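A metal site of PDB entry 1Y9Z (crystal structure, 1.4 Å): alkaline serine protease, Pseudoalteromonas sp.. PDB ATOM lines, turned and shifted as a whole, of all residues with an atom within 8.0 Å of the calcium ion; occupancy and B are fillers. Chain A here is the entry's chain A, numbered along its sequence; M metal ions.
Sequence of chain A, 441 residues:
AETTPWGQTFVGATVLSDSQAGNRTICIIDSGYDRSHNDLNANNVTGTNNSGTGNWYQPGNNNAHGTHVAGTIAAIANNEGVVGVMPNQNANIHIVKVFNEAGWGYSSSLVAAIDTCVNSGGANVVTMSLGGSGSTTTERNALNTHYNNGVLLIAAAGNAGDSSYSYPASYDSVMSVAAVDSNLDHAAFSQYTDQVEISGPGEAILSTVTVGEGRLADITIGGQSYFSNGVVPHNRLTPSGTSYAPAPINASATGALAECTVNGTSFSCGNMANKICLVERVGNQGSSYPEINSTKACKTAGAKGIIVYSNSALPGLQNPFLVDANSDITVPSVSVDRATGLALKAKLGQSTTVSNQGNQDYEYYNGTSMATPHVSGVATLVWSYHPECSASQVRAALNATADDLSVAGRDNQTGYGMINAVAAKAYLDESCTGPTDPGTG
Within 4 Å of the calcium ion: Glu 2, Asp 39, Ile 76, Asn 78, Glu 80 and Val 82.
The calcium ion is bound by the backbone carbonyl oxygen (O) of Glu 80, the backbone carbonyl oxygen (O) of Ile 76, the side-chain carboxylate (OE1) of Glu 2, the backbone carbonyl oxygen (O) of Val 82, the side-chain amide oxygen (OD1) of Asn 78, the side-chain carboxylate (OD1) of Asp 39 and the side-chain carboxylate (OD2) of Asp 39.
OE1 of Glu 2 lies close to N of Asn 79.
The side-chain amide nitrogen (ND2) of Asn 38 lies within hydrogen-bond range of the side-chain carboxylate (OE1) of Glu 80 (3.4 Å).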
ATOM      1  N   ALA A   1     -24.419 -23.102   3.188  1.00  0.00           N
ATOM      2  CA  ALA A   1     -23.227 -23.634   3.902  1.00  0.00           C
ATOM      3  C   ALA A   1     -23.072 -22.938   5.250  1.00  0.00           C
ATOM      4  O   ALA A   1     -23.420 -21.765   5.399  1.00  0.00           O
ATOM      5  CB  ALA A   1     -21.976 -23.421   3.059  1.00  0.00           C
ATOM      6  N   GLU A   2     -22.555 -23.665   6.227  1.00  0.00           N
ATOM      7  CA  GLU A   2     -22.358 -23.131   7.572  1.00  0.00           C
ATOM      8  C   GLU A   2     -20.882 -23.222   7.936  1.00  0.00           C
ATOM      9  O   GLU A   2     -20.249 -24.260   7.740  1.00  0.00           O
ATOM     10  CB  GLU A   2     -23.208 -23.914   8.565  1.00  0.00           C
ATOM     11  CG  GLU A   2     -23.062 -23.488  10.012  1.00  0.00           C
ATOM     12  CD  GLU A   2     -24.104 -24.144  10.889  1.00  0.00           C
ATOM     13  OE1 GLU A   2     -25.124 -23.485  11.202  1.00  0.00           O
ATOM     14  OE2 GLU A   2     -23.923 -25.325  11.244  1.00  0.00           O
ATOM     15  N   THR A   3     -20.340 -22.128   8.454  1.00  0.00           N
ATOM     16  CA  THR A   3     -18.935 -22.072   8.835  1.00  0.00           C
ATOM     17  C   THR A   3     -18.735 -22.095  10.343  1.00  0.00           C
ATOM     18  O   THR A   3     -19.549 -21.560  11.100  1.00  0.00           O
ATOM     19  CB  THR A   3     -18.268 -20.801   8.268  1.00  0.00           C
ATOM     20  OG1 THR A   3     -18.265 -20.858   6.832  1.00  0.00           O
ATOM     21  CG2 THR A   3     -16.830 -20.677   8.761  1.00  0.00           C
ATOM     22  N   HIS A  37     -33.020 -12.601  13.174  1.00  0.00           N
ATOM     23  CA  HIS A  37     -31.914 -13.263  12.489  1.00  0.00           C
ATOM     24  C   HIS A  37     -32.109 -14.776  12.423  1.00  0.00           C
ATOM     25  O   HIS A  37     -32.448 -15.405  13.423  1.00  0.00           O
ATOM     26  CB  HIS A  37     -30.595 -12.944  13.210  1.00  0.00           C
ATOM     27  CG  HIS A  37     -29.381 -13.299  12.429  1.00  0.00           C
ATOM     28  ND1 HIS A  37     -28.441 -12.366  12.034  1.00  0.00           N
ATOM     29  CD2 HIS A  37     -28.953 -14.483  11.930  1.00  0.00           C
ATOM     30  CE1 HIS A  37     -27.491 -12.964  11.332  1.00  0.00           C
ATOM     31  NE2 HIS A  37     -27.777 -14.248  11.263  1.00  0.00           N
ATOM     32  N   ASN A  38     -31.886 -15.367  11.253  1.00  0.00           N
ATOM     33  CA  ASN A  38     -32.064 -16.807  11.073  1.00  0.00           C
ATOM     34  C   ASN A  38     -31.221 -17.666  11.998  1.00  0.00           C
ATOM     35  O   ASN A  38     -31.622 -18.775  12.357  1.00  0.00           O
ATOM     36  CB  ASN A  38     -31.783 -17.218   9.625  1.00  0.00           C
ATOM     37  CG  ASN A  38     -32.820 -16.713   8.641  1.00  0.00           C
ATOM     38  OD1 ASN A  38     -33.939 -16.365   9.025  1.00  0.00           O
ATOM     39  ND2 ASN A  38     -32.462 -16.683   7.364  1.00  0.00           N
ATOM     40  N   ASP A  39     -30.051 -17.175  12.383  1.00  0.00           N
ATOM     41  CA  ASP A  39     -29.173 -17.943  13.272  1.00  0.00           C
ATOM     42  C   ASP A  39     -29.416 -17.669  14.750  1.00  0.00           C
ATOM     43  O   ASP A  39     -28.696 -18.178  15.602  1.00  0.00           O
ATOM     44  CB  ASP A  39     -27.698 -17.654  12.925  1.00  0.00           C
ATOM     45  CG  ASP A  39     -27.040 -18.799  12.176  1.00  0.00           C
ATOM     46  OD1 ASP A  39     -27.765 -19.651  11.623  1.00  0.00           O
ATOM     47  OD2 ASP A  39     -25.784 -18.845  12.129  1.00  0.00           O
ATOM     48  N   LEU A  40     -30.455 -16.877  15.048  1.00  0.00           N
ATOM     49  CA  LEU A  40     -30.770 -16.538  16.438  1.00  0.00           C
ATOM     50  C   LEU A  40     -32.243 -16.625  16.809  1.00  0.00           C
ATOM     51  O   LEU A  40     -32.587 -16.722  17.982  1.00  0.00           O
ATOM     52  CB  LEU A  40     -30.284 -15.125  16.752  1.00  0.00           C
ATOM     53  CG  LEU A  40     -28.786 -14.838  16.684  1.00  0.00           C
ATOM     54  CD1 LEU A  40     -28.542 -13.347  16.861  1.00  0.00           C
ATOM     55  CD2 LEU A  40     -28.065 -15.636  17.770  1.00  0.00           C
ATOM     56  N   ALA A  74     -24.385 -18.643  21.030  1.00  0.00           N
ATOM     57  CA  ALA A  74     -25.377 -19.594  20.552  1.00  0.00           C
ATOM     58  C   ALA A  74     -25.910 -19.488  19.125  1.00  0.00           C
ATOM     59  O   ALA A  74     -27.080 -19.773  18.899  1.00  0.00           O
ATOM     60  CB  ALA A  74     -26.542 -19.616  21.531  1.00  0.00           C
ATOM     61  N   ALA A  75     -25.087 -19.061  18.174  1.00  0.00           N
ATOM     62  CA  ALA A  75     -25.576 -19.020  16.788  1.00  0.00           C
ATOM     63  C   ALA A  75     -26.043 -20.451  16.506  1.00  0.00           C
ATOM     64  O   ALA A  75     -25.330 -21.412  16.797  1.00  0.00           O
ATOM     65  CB  ALA A  75     -24.468 -18.605  15.841  1.00  0.00           C
ATOM     66  N   ILE A  76     -27.228 -20.579  15.930  1.00  0.00           N
ATOM     67  CA  ILE A  76     -27.823 -21.882  15.666  1.00  0.00           C
ATOM     68  C   ILE A  76     -27.204 -22.735  14.566  1.00  0.00           C
ATOM     69  O   ILE A  76     -26.851 -22.241  13.504  1.00  0.00           O
ATOM     70  CB  ILE A  76     -29.324 -21.713  15.371  1.00  0.00           C
ATOM     71  CG1 ILE A  76     -29.998 -21.030  16.576  1.00  0.00           C
ATOM     72  CG2 ILE A  76     -29.980 -23.056  15.103  1.00  0.00           C
ATOM     73  CD1 ILE A  76     -31.432 -20.648  16.331  1.00  0.00           C
ATOM     74  N   ALA A  77     -27.070 -24.026  14.844  1.00  0.00           N
ATOM     75  CA  ALA A  77     -26.531 -24.980  13.878  1.00  0.00           C
ATOM     76  C   ALA A  77     -27.660 -25.276  12.883  1.00  0.00           C
ATOM     77  O   ALA A  77     -28.713 -25.796  13.280  1.00  0.00           O
ATOM     78  CB  ALA A  77     -26.103 -26.260  14.596  1.00  0.00           C
ATOM     79  N   ASN A  78     -27.439 -24.931  11.625  1.00  0.00           N
ATOM     80  CA  ASN A  78     -28.478 -25.118  10.616  1.00  0.00           C
ATOM     81  C   ASN A  78     -27.989 -25.039   9.169  1.00  0.00           C
ATOM     82  O   ASN A  78     -28.751 -24.661   8.274  1.00  0.00           O
ATOM     83  CB  ASN A  78     -29.570 -24.069  10.821  1.00  0.00           C
ATOM     84  CG  ASN A  78     -29.002 -22.665  10.884  1.00  0.00           C
ATOM     85  OD1 ASN A  78     -27.859 -22.425  10.484  1.00  0.00           O
ATOM     86  ND2 ASN A  78     -29.799 -21.710  11.381  1.00  0.00           N
ATOM     87  N   ASN A  79     -26.731 -25.381   8.919  1.00  0.00           N
ATOM     88  CA  ASN A  79     -26.214 -25.344   7.549  1.00  0.00           C
ATOM     89  C   ASN A  79     -26.173 -23.945   6.885  1.00  0.00           C
ATOM     90  O   ASN A  79     -26.052 -23.843   5.654  1.00  0.00           O
ATOM     91  CB  ASN A  79     -27.024 -26.307   6.664  1.00  0.00           C
ATOM     92  CG  ASN A  79     -26.382 -26.526   5.297  1.00  0.00           C
ATOM     93  OD1 ASN A  79     -25.223 -26.928   5.193  1.00  0.00           O
ATOM     94  ND2 ASN A  79     -27.145 -26.276   4.237  1.00  0.00           N
ATOM     95  N   GLU A  80     -26.301 -22.885   7.677  1.00  0.00           N
ATOM     96  CA  GLU A  80     -26.211 -21.512   7.155  1.00  0.00           C
ATOM     97  C   GLU A  80     -25.523 -20.656   8.208  1.00  0.00           C
ATOM     98  O   GLU A  80     -25.567 -20.972   9.397  1.00  0.00           O
ATOM     99  CB  GLU A  80     -27.596 -20.932   6.830  1.00  0.00           C
ATOM    100  CG  GLU A  80     -28.443 -20.519   8.020  1.00  0.00           C
ATOM    101  CD  GLU A  80     -29.745 -19.819   7.610  1.00  0.00           C
ATOM    102  OE1 GLU A  80     -29.683 -18.648   7.160  1.00  0.00           O
ATOM    103  OE2 GLU A  80     -30.812 -20.446   7.720  1.00  0.00           O
ATOM    104  N   GLY A  81     -24.861 -19.598   7.768  1.00  0.00           N
ATOM    105  CA  GLY A  81     -24.184 -18.725   8.709  1.00  0.00           C
ATOM    106  C   GLY A  81     -23.057 -19.377   9.492  1.00  0.00           C
ATOM    107  O   GLY A  81     -22.136 -19.949   8.920  1.00  0.00           O
ATOM    108  N   VAL A  82     -23.146 -19.294  10.820  1.00  0.00           N
ATOM    109  CA  VAL A  82     -22.129 -19.864  11.688  1.00  0.00           C
ATOM    110  C   VAL A  82     -22.752 -20.697  12.800  1.00  0.00           C
ATOM    111  O   VAL A  82     -23.932 -21.051  12.741  1.00  0.00           O
ATOM    112  CB  VAL A  82     -21.258 -18.737  12.321  1.00  0.00           C
ATOM    113  CG1 VAL A  82     -20.553 -17.945  11.236  1.00  0.00           C
ATOM    114  CG2 VAL A  82     -22.131 -17.811  13.154  1.00  0.00           C
ATOM    115  N   VAL A  83     -21.938 -21.036  13.802  1.00  0.00           N
ATOM    116  CA  VAL A  83     -22.384 -21.797  14.958  1.00  0.00           C
ATOM    117  C   VAL A  83     -21.719 -21.209  16.203  1.00  0.00           C
ATOM    118  O   VAL A  83     -20.566 -20.785  16.150  1.00  0.00           O
ATOM    119  CB  VAL A  83     -22.003 -23.297  14.863  1.00  0.00           C
ATOM    120  CG1 VAL A  83     -22.790 -23.965  13.751  1.00  0.00           C
ATOM    121  CG2 VAL A  83     -20.512 -23.453  14.602  1.00  0.00           C
ATOM    122  N   GLY A  84     -22.470 -21.164  17.303  1.00  0.00           N
ATOM    123  CA  GLY A  84     -21.935 -20.651  18.542  1.00  0.00           C
ATOM    124  C   GLY A  84     -21.482 -21.785  19.445  1.00  0.00           C
ATOM    125  O   GLY A  84     -21.547 -22.953  19.056  1.00  0.00           O
ATOM    126  N   PRO A  87     -24.849 -24.350  20.004  1.00  0.00           N
ATOM    127  CA  PRO A  87     -25.674 -24.154  18.813  1.00  0.00           C
ATOM    128  C   PRO A  87     -26.918 -25.012  18.592  1.00  0.00           C
ATOM    129  O   PRO A  87     -27.610 -24.836  17.584  1.00  0.00           O
ATOM    130  CB  PRO A  87     -24.680 -24.383  17.705  1.00  0.00           C
ATOM    131  CG  PRO A  87     -23.971 -25.617  18.225  1.00  0.00           C
ATOM    132  CD  PRO A  87     -23.769 -25.318  19.721  1.00  0.00           C
ATOM    133  N   THR A 208     -22.785 -13.370  14.088  1.00  0.00           N
ATOM    134  CA  THR A 208     -24.027 -12.768  13.647  1.00  0.00           C
ATOM    135  C   THR A 208     -24.095 -11.283  13.988  1.00  0.00           C
ATOM    136  O   THR A 208     -23.566 -10.851  15.015  1.00  0.00           O
ATOM    137  CB  THR A 208     -25.225 -13.438  14.348  1.00  0.00           C
ATOM    138  OG1 THR A 208     -24.976 -13.468  15.761  1.00  0.00           O
ATOM    139  CG2 THR A 208     -25.425 -14.862  13.849  1.00  0.00           C
ATOM    140  N   TYR A 362     -23.588 -11.171   8.832  1.00  0.00           N
ATOM    141  CA  TYR A 362     -22.477 -11.634   9.673  1.00  0.00           C
ATOM    142  C   TYR A 362     -21.338 -10.659   9.470  1.00  0.00           C
ATOM    143  O   TYR A 362     -21.302  -9.927   8.482  1.00  0.00           O
ATOM    144  CB  TYR A 362     -22.045 -13.035   9.252  1.00  0.00           C
ATOM    145  CG  TYR A 362     -23.165 -14.037   9.263  1.00  0.00           C
ATOM    146  CD1 TYR A 362     -23.476 -14.753  10.424  1.00  0.00           C
ATOM    147  CD2 TYR A 362     -23.968 -14.214   8.147  1.00  0.00           C
ATOM    148  CE1 TYR A 362     -24.561 -15.617  10.458  1.00  0.00           C
ATOM    149  CE2 TYR A 362     -25.062 -15.070   8.177  1.00  0.00           C
ATOM    150  CZ  TYR A 362     -25.357 -15.773   9.326  1.00  0.00           C
ATOM    151  OH  TYR A 362     -26.447 -16.595   9.366  1.00  0.00           O
HETATM  152 CA    CA M   1     -25.997 -21.350  11.574  1.00  0.00          CA
